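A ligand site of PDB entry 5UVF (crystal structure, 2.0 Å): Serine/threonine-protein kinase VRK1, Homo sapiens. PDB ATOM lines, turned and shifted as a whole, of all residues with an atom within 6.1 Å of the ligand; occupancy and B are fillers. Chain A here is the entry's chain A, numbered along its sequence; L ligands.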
ATOM      1  N   ILE A  43     -20.499   5.365 -12.668  1.00  0.00           N
ATOM      2  CA  ILE A  43     -19.205   5.064 -12.104  1.00  0.00           C
ATOM      3  C   ILE A  43     -19.107   5.670 -10.712  1.00  0.00           C
ATOM      4  O   ILE A  43     -20.062   6.292 -10.241  1.00  0.00           O
ATOM      5  CB  ILE A  43     -18.034   5.590 -12.958  1.00  0.00           C
ATOM      6  CG1 ILE A  43     -18.263   7.044 -13.332  1.00  0.00           C
ATOM      7  CG2 ILE A  43     -17.859   4.735 -14.200  1.00  0.00           C
ATOM      8  CD1 ILE A  43     -17.128   7.620 -14.137  1.00  0.00           C
ATOM      9  N   GLY A  49     -22.130  12.297  -8.019  1.00  0.00           N
ATOM     10  CA  GLY A  49     -23.199  11.351  -7.757  1.00  0.00           C
ATOM     11  C   GLY A  49     -23.750  10.750  -9.030  1.00  0.00           C
ATOM     12  O   GLY A  49     -23.465   9.602  -9.356  1.00  0.00           O
ATOM     13  N   ILE A  51     -23.180  10.430 -12.260  1.00  0.00           N
ATOM     14  CA  ILE A  51     -22.167  10.500 -13.296  1.00  0.00           C
ATOM     15  C   ILE A  51     -22.098   9.160 -13.997  1.00  0.00           C
ATOM     16  O   ILE A  51     -22.061   8.120 -13.362  1.00  0.00           O
ATOM     17  CB  ILE A  51     -20.791  10.814 -12.697  1.00  0.00           C
ATOM     18  CG1 ILE A  51     -20.825  12.166 -11.977  1.00  0.00           C
ATOM     19  CG2 ILE A  51     -19.728  10.821 -13.777  1.00  0.00           C
ATOM     20  CD1 ILE A  51     -19.578  12.450 -11.164  1.00  0.00           C
ATOM     21  N   VAL A  69     -17.034  11.165 -19.391  1.00  0.00           N
ATOM     22  CA  VAL A  69     -18.068  11.037 -18.382  1.00  0.00           C
ATOM     23  C   VAL A  69     -19.156  12.047 -18.717  1.00  0.00           C
ATOM     24  O   VAL A  69     -18.875  13.088 -19.310  1.00  0.00           O
ATOM     25  CB  VAL A  69     -17.621  11.141 -16.887  1.00  0.00           C
ATOM     26  CG1 VAL A  69     -16.669  10.005 -16.509  1.00  0.00           C
ATOM     27  CG2 VAL A  69     -17.029  12.508 -16.539  1.00  0.00           C
ATOM     28  N   LYS A  71     -22.082  14.079 -16.615  1.00  0.00           N
ATOM     29  CA  LYS A  71     -22.614  14.461 -15.292  1.00  0.00           C
ATOM     30  C   LYS A  71     -24.001  15.042 -15.599  1.00  0.00           C
ATOM     31  O   LYS A  71     -24.144  15.818 -16.548  1.00  0.00           O
ATOM     32  CB  LYS A  71     -21.701  15.512 -14.631  1.00  0.00           C
ATOM     33  N   GLU A  83     -20.479  25.330 -12.428  1.00  0.00           N
ATOM     34  CA  GLU A  83     -19.419  24.515 -12.992  1.00  0.00           C
ATOM     35  C   GLU A  83     -19.370  24.634 -14.512  1.00  0.00           C
ATOM     36  O   GLU A  83     -18.310  24.801 -15.097  1.00  0.00           O
ATOM     37  CB  GLU A  83     -19.601  23.060 -12.580  1.00  0.00           C
ATOM     38  CG  GLU A  83     -18.485  22.142 -13.034  1.00  0.00           C
ATOM     39  CD  GLU A  83     -18.387  20.880 -12.215  1.00  0.00           C
ATOM     40  OE1 GLU A  83     -19.403  20.193 -12.052  1.00  0.00           O
ATOM     41  OE2 GLU A  83     -17.290  20.576 -11.724  1.00  0.00           O
ATOM     42  N   TYR A  87     -16.299  26.010 -17.024  1.00  0.00           N
ATOM     43  CA  TYR A  87     -15.800  25.230 -18.139  1.00  0.00           C
ATOM     44  C   TYR A  87     -15.975  25.954 -19.478  1.00  0.00           C
ATOM     45  O   TYR A  87     -15.055  26.011 -20.263  1.00  0.00           O
ATOM     46  CB  TYR A  87     -16.416  23.832 -18.137  1.00  0.00           C
ATOM     47  CG  TYR A  87     -15.787  22.904 -17.114  1.00  0.00           C
ATOM     48  CD1 TYR A  87     -14.445  22.617 -17.163  1.00  0.00           C
ATOM     49  CD2 TYR A  87     -16.527  22.320 -16.107  1.00  0.00           C
ATOM     50  CE1 TYR A  87     -13.842  21.792 -16.249  1.00  0.00           C
ATOM     51  CE2 TYR A  87     -15.939  21.484 -15.180  1.00  0.00           C
ATOM     52  CZ  TYR A  87     -14.590  21.225 -15.257  1.00  0.00           C
ATOM     53  OH  TYR A  87     -13.966  20.402 -14.364  1.00  0.00           O
ATOM     54  N   PRO A 111      -9.454  19.933 -16.340  1.00  0.00           N
ATOM     55  CA  PRO A 111     -10.182  18.957 -17.153  1.00  0.00           C
ATOM     56  C   PRO A 111     -10.782  19.557 -18.422  1.00  0.00           C
ATOM     57  O   PRO A 111     -11.186  20.700 -18.425  1.00  0.00           O
ATOM     58  CB  PRO A 111     -11.303  18.488 -16.221  1.00  0.00           C
ATOM     59  CG  PRO A 111     -10.817  18.800 -14.852  1.00  0.00           C
ATOM     60  CD  PRO A 111     -10.031  20.069 -15.005  1.00  0.00           C
ATOM     61  N   LYS A 112     -10.842  18.773 -19.488  1.00  0.00           N
ATOM     62  CA  LYS A 112     -11.429  19.310 -20.719  1.00  0.00           C
ATOM     63  C   LYS A 112     -12.936  19.165 -20.733  1.00  0.00           C
ATOM     64  O   LYS A 112     -13.483  18.129 -20.350  1.00  0.00           O
ATOM     65  CB  LYS A 112     -10.778  18.745 -21.982  1.00  0.00           C
ATOM     66  CG  LYS A 112      -9.449  19.455 -22.274  1.00  0.00           C
ATOM     67  CD  LYS A 112      -8.797  18.997 -23.576  1.00  0.00           C
ATOM     68  CE  LYS A 112      -7.469  19.681 -23.798  1.00  0.00           C
ATOM     69  NZ  LYS A 112      -6.391  19.111 -22.927  1.00  0.00           N
ATOM     70  N   MET A 129     -23.392  17.514 -18.861  1.00  0.00           N
ATOM     71  CA  MET A 129     -22.127  18.080 -19.280  1.00  0.00           C
ATOM     72  C   MET A 129     -21.177  16.918 -19.527  1.00  0.00           C
ATOM     73  O   MET A 129     -21.140  15.979 -18.731  1.00  0.00           O
ATOM     74  CB  MET A 129     -21.615  18.988 -18.120  1.00  0.00           C
ATOM     75  CG  MET A 129     -20.300  19.686 -18.398  1.00  0.00           C
ATOM     76  SD  MET A 129     -19.867  20.785 -16.988  1.00  0.00           S
ATOM     77  CE  MET A 129     -19.390  19.588 -15.739  1.00  0.00           C
ATOM     78  N   MET A 131     -17.384  15.560 -19.929  1.00  0.00           N
ATOM     79  CA  MET A 131     -16.043  15.862 -19.461  1.00  0.00           C
ATOM     80  C   MET A 131     -15.087  14.692 -19.654  1.00  0.00           C
ATOM     81  O   MET A 131     -15.501  13.578 -19.953  1.00  0.00           O
ATOM     82  CB  MET A 131     -16.075  16.119 -17.957  1.00  0.00           C
ATOM     83  CG  MET A 131     -17.099  17.130 -17.507  1.00  0.00           C
ATOM     84  SD  MET A 131     -16.568  18.742 -18.061  1.00  0.00           S
ATOM     85  CE  MET A 131     -14.876  18.711 -17.514  1.00  0.00           C
ATOM     86  N   ASP A 132     -13.821  14.968 -19.428  1.00  0.00           N
ATOM     87  CA  ASP A 132     -12.773  13.981 -19.503  1.00  0.00           C
ATOM     88  C   ASP A 132     -13.000  12.937 -18.423  1.00  0.00           C
ATOM     89  O   ASP A 132     -13.418  13.259 -17.321  1.00  0.00           O
ATOM     90  CB  ASP A 132     -11.435  14.633 -19.179  1.00  0.00           C
ATOM     91  CG  ASP A 132     -10.729  15.155 -20.397  1.00  0.00           C
ATOM     92  OD1 ASP A 132     -10.879  14.564 -21.483  1.00  0.00           O
ATOM     93  OD2 ASP A 132      -9.988  16.150 -20.260  1.00  0.00           O
ATOM     94  N   ARG A 133     -12.708  11.697 -18.736  1.00  0.00           N
ATOM     95  CA  ARG A 133     -12.815  10.625 -17.782  1.00  0.00           C
ATOM     96  C   ARG A 133     -11.442  10.525 -17.147  1.00  0.00           C
ATOM     97  O   ARG A 133     -10.431  10.678 -17.811  1.00  0.00           O
ATOM     98  CB  ARG A 133     -13.199   9.311 -18.453  1.00  0.00           C
ATOM     99  CG  ARG A 133     -13.377   8.157 -17.479  1.00  0.00           C
ATOM    100  CD  ARG A 133     -12.194   7.207 -17.551  1.00  0.00           C
ATOM    101  NE  ARG A 133     -12.294   6.134 -16.577  1.00  0.00           N
ATOM    102  CZ  ARG A 133     -12.872   4.959 -16.810  1.00  0.00           C
ATOM    103  NH1 ARG A 133     -13.400   4.709 -17.999  1.00  0.00           N
ATOM    104  NH2 ARG A 133     -12.913   4.038 -15.864  1.00  0.00           N
ATOM    105  N   PHE A 134     -11.419  10.257 -15.856  1.00  0.00           N
ATOM    106  CA  PHE A 134     -10.160  10.159 -15.160  1.00  0.00           C
ATOM    107  C   PHE A 134     -10.004   8.841 -14.440  1.00  0.00           C
ATOM    108  O   PHE A 134     -10.858   7.983 -14.448  1.00  0.00           O
ATOM    109  CB  PHE A 134      -9.999  11.306 -14.157  1.00  0.00           C
ATOM    110  CG  PHE A 134      -9.886  12.645 -14.788  1.00  0.00           C
ATOM    111  CD1 PHE A 134      -8.740  13.011 -15.445  1.00  0.00           C
ATOM    112  CD2 PHE A 134     -10.942  13.527 -14.748  1.00  0.00           C
ATOM    113  CE1 PHE A 134      -8.636  14.248 -16.049  1.00  0.00           C
ATOM    114  CE2 PHE A 134     -10.845  14.757 -15.350  1.00  0.00           C
ATOM    115  CZ  PHE A 134      -9.691  15.119 -15.996  1.00  0.00           C
ATOM    116  N   GLY A 135      -8.851   8.711 -13.839  1.00  0.00           N
ATOM    117  CA  GLY A 135      -8.497   7.581 -13.012  1.00  0.00           C
ATOM    118  C   GLY A 135      -8.776   7.865 -11.548  1.00  0.00           C
ATOM    119  O   GLY A 135      -9.616   8.665 -11.175  1.00  0.00           O
ATOM    120  N   SER A 136      -8.088   7.144 -10.682  1.00  0.00           N
ATOM    121  CA  SER A 136      -8.297   7.318  -9.250  1.00  0.00           C
ATOM    122  C   SER A 136      -8.024   8.725  -8.729  1.00  0.00           C
ATOM    123  O   SER A 136      -7.328   9.510  -9.365  1.00  0.00           O
ATOM    124  CB  SER A 136      -7.411   6.317  -8.495  1.00  0.00           C
ATOM    125  OG  SER A 136      -7.649   6.350  -7.099  1.00  0.00           O
ATOM    126  N   LYS A 140      -7.558   8.280  -2.343  1.00  0.00           N
ATOM    127  CA  LYS A 140      -7.468   6.830  -2.292  1.00  0.00           C
ATOM    128  C   LYS A 140      -6.008   6.357  -2.240  1.00  0.00           C
ATOM    129  O   LYS A 140      -5.666   5.493  -1.452  1.00  0.00           O
ATOM    130  CB  LYS A 140      -8.162   6.205  -3.497  1.00  0.00           C
ATOM    131  CG  LYS A 140      -9.667   6.390  -3.535  1.00  0.00           C
ATOM    132  CD  LYS A 140     -10.268   5.758  -4.790  1.00  0.00           C
ATOM    133  CE  LYS A 140     -11.780   5.922  -4.823  1.00  0.00           C
ATOM    134  NZ  LYS A 140     -12.409   5.328  -6.046  1.00  0.00           N
ATOM    135  N   SER A 181      -9.173  14.503  -2.584  1.00  0.00           N
ATOM    136  CA  SER A 181     -10.331  13.858  -3.239  1.00  0.00           C
ATOM    137  C   SER A 181     -10.768  14.613  -4.496  1.00  0.00           C
ATOM    138  O   SER A 181     -11.493  14.043  -5.323  1.00  0.00           O
ATOM    139  CB  SER A 181     -11.500  13.684  -2.271  1.00  0.00           C
ATOM    140  OG  SER A 181     -11.977  14.944  -1.830  1.00  0.00           O
ATOM    141  N   ASN A 182     -10.278  15.863  -4.676  1.00  0.00           N
ATOM    142  CA  ASN A 182     -10.546  16.730  -5.837  1.00  0.00           C
ATOM    143  C   ASN A 182      -9.406  16.736  -6.834  1.00  0.00           C
ATOM    144  O   ASN A 182      -9.386  17.536  -7.768  1.00  0.00           O
ATOM    145  CB  ASN A 182     -10.930  18.151  -5.366  1.00  0.00           C
ATOM    146  CG  ASN A 182     -12.376  18.234  -4.932  1.00  0.00           C
ATOM    147  OD1 ASN A 182     -13.192  17.356  -5.265  1.00  0.00           O
ATOM    148  ND2 ASN A 182     -12.737  19.260  -4.181  1.00  0.00           N
ATOM    149  N   LEU A 184      -7.504  14.259  -9.467  1.00  0.00           N
ATOM    150  CA  LEU A 184      -7.667  13.006 -10.204  1.00  0.00           C
ATOM    151  C   LEU A 184      -6.508  12.765 -11.167  1.00  0.00           C
ATOM    152  O   LEU A 184      -5.981  13.713 -11.743  1.00  0.00           O
ATOM    153  CB  LEU A 184      -9.011  13.073 -10.965  1.00  0.00           C
ATOM    154  CG  LEU A 184     -10.314  12.522 -10.292  1.00  0.00           C
ATOM    155  CD1 LEU A 184     -10.501  12.950  -8.865  1.00  0.00           C
ATOM    156  CD2 LEU A 184     -11.585  12.932 -11.081  1.00  0.00           C
ATOM    157  N   VAL A 196     -10.383  18.958 -10.093  1.00  0.00           N
ATOM    158  CA  VAL A 196     -11.802  18.840 -10.506  1.00  0.00           C
ATOM    159  C   VAL A 196     -12.711  19.537  -9.496  1.00  0.00           C
ATOM    160  O   VAL A 196     -12.259  19.929  -8.407  1.00  0.00           O
ATOM    161  CB  VAL A 196     -12.247  17.355 -10.718  1.00  0.00           C
ATOM    162  CG1 VAL A 196     -11.394  16.650 -11.757  1.00  0.00           C
ATOM    163  CG2 VAL A 196     -12.263  16.560  -9.403  1.00  0.00           C
ATOM    164  N   ASP A 197     -13.988  19.574  -9.866  1.00  0.00           N
ATOM    165  CA  ASP A 197     -15.115  20.154  -9.116  1.00  0.00           C
ATOM    166  C   ASP A 197     -15.100  21.678  -9.021  1.00  0.00           C
ATOM    167  O   ASP A 197     -14.481  22.254  -8.144  1.00  0.00           O
ATOM    168  CB  ASP A 197     -15.350  19.467  -7.759  1.00  0.00           C
ATOM    169  CG  ASP A 197     -16.612  19.924  -7.060  1.00  0.00           C
ATOM    170  OD1 ASP A 197     -17.331  20.776  -7.599  1.00  0.00           O
ATOM    171  OD2 ASP A 197     -16.872  19.417  -5.967  1.00  0.00           O
ATOM    172  N   TYR A 198     -15.795  22.328  -9.962  1.00  0.00           N
ATOM    173  CA  TYR A 198     -15.864  23.765  -9.978  1.00  0.00           C
ATOM    174  C   TYR A 198     -17.292  24.230  -9.645  1.00  0.00           C
ATOM    175  O   TYR A 198     -17.623  25.390  -9.859  1.00  0.00           O
ATOM    176  CB  TYR A 198     -15.298  24.317 -11.309  1.00  0.00           C
ATOM    177  CG  TYR A 198     -13.820  24.008 -11.517  1.00  0.00           C
ATOM    178  CD1 TYR A 198     -13.406  22.770 -12.016  1.00  0.00           C
ATOM    179  CD2 TYR A 198     -12.848  24.951 -11.210  1.00  0.00           C
ATOM    180  CE1 TYR A 198     -12.063  22.471 -12.166  1.00  0.00           C
ATOM    181  CE2 TYR A 198     -11.483  24.667 -11.385  1.00  0.00           C
ATOM    182  CZ  TYR A 198     -11.098  23.412 -11.838  1.00  0.00           C
ATOM    183  OH  TYR A 198      -9.776  23.109 -12.028  1.00  0.00           O
HETATM  184  C1  LIG L   1     -13.292   6.821 -11.770  1.00  0.00           C
HETATM  185  C2  LIG L   1     -14.715  16.169 -14.135  1.00  0.00           C
HETATM  186  C3  LIG L   1     -14.203  14.943 -14.471  1.00  0.00           C
HETATM  187  C4  LIG L   1     -15.733  16.312 -13.208  1.00  0.00           C
HETATM  188  C5  LIG L   1     -16.226  15.171 -12.611  1.00  0.00           C
HETATM  189  N1  LIG L   1     -13.591  10.387 -14.013  1.00  0.00           N
HETATM  190  C6  LIG L   1     -15.743  13.926 -12.911  1.00  0.00           C
HETATM  191  C7  LIG L   1     -14.731  13.818 -13.848  1.00  0.00           C
HETATM  192  C8  LIG L   1     -16.540  13.235  -7.834  1.00  0.00           C
HETATM  193  C9  LIG L   1     -15.210  13.561  -8.469  1.00  0.00           C
HETATM  194  C10 LIG L   1     -15.343  14.759  -9.395  1.00  0.00           C
HETATM  195  C11 LIG L   1     -14.666  12.354  -9.233  1.00  0.00           C
HETATM  196  C12 LIG L   1     -15.766  11.353  -9.546  1.00  0.00           C
HETATM  197  C13 LIG L   1     -14.822  10.257 -11.568  1.00  0.00           C
HETATM  198  C14 LIG L   1     -14.226  11.420 -13.441  1.00  0.00           C
HETATM  199  C15 LIG L   1     -13.582   9.254 -13.343  1.00  0.00           C
HETATM  200  O1  LIG L   1     -16.230  17.519 -12.888  1.00  0.00           O
HETATM  201  C16 LIG L   1     -14.188   9.123 -12.082  1.00  0.00           C
HETATM  202  C17 LIG L   1     -14.940   7.720 -10.239  1.00  0.00           C
HETATM  203  C18 LIG L   1     -15.877   8.857  -9.863  1.00  0.00           C
HETATM  204  N2  LIG L   1     -14.859  11.420 -12.236  1.00  0.00           N
HETATM  205  F1  LIG L   1     -17.216  15.292 -11.709  1.00  0.00           F
HETATM  206  F2  LIG L   1     -14.222  17.264 -14.740  1.00  0.00           F
HETATM  207  N3  LIG L   1     -14.206  12.551 -14.173  1.00  0.00           N
HETATM  208  N4  LIG L   1     -14.173   7.911 -11.350  1.00  0.00           N
HETATM  209  O2  LIG L   1     -14.874   6.691  -9.617  1.00  0.00           O
HETATM  210  N5  LIG L   1     -15.455  10.173 -10.351  1.00  0.00           N
HETATM  211  C19 LIG L   1     -17.304   8.519 -10.249  1.00  0.00           C
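The backbone NH (N) of Phe 134 lies within hydrogen-bond range of a nitrogen (N1) of the ligand. A nitrogen (N3) of the ligand lies within hydrogen-bond range of the backbone carbonyl oxygen (O) of Asp 132. OE2 of Glu 83 sits at hydrogen-bond distance from O1 of the ligand (3.4 Å).
O of Met 131 lies within hydrogen-bond range of N of Val 69. OD2 of Asp 132 lies within hydrogen-bond range of N of Lys 112, 2.9 Å away. N of Ile 43 sits at hydrogen-bond distance from O of Ile 51, 3.2 Å away. OE2 of Glu 83 is in hydrogen-bond range of N of Tyr 198, at 2.9 Å. The backbone NH (N) of Val 196 lies within hydrogen-bond range of the backbone carbonyl oxygen (O) of Asn 182.
The side-chain hydroxyl (OH) of Tyr 87 lies close to a fluorine (F2) of the ligand. Merely in contact with the ligand: Ile 43, Ile 51, Val 69, Pro 111, Met 131, Arg 133, Leu 184 and Val 196.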
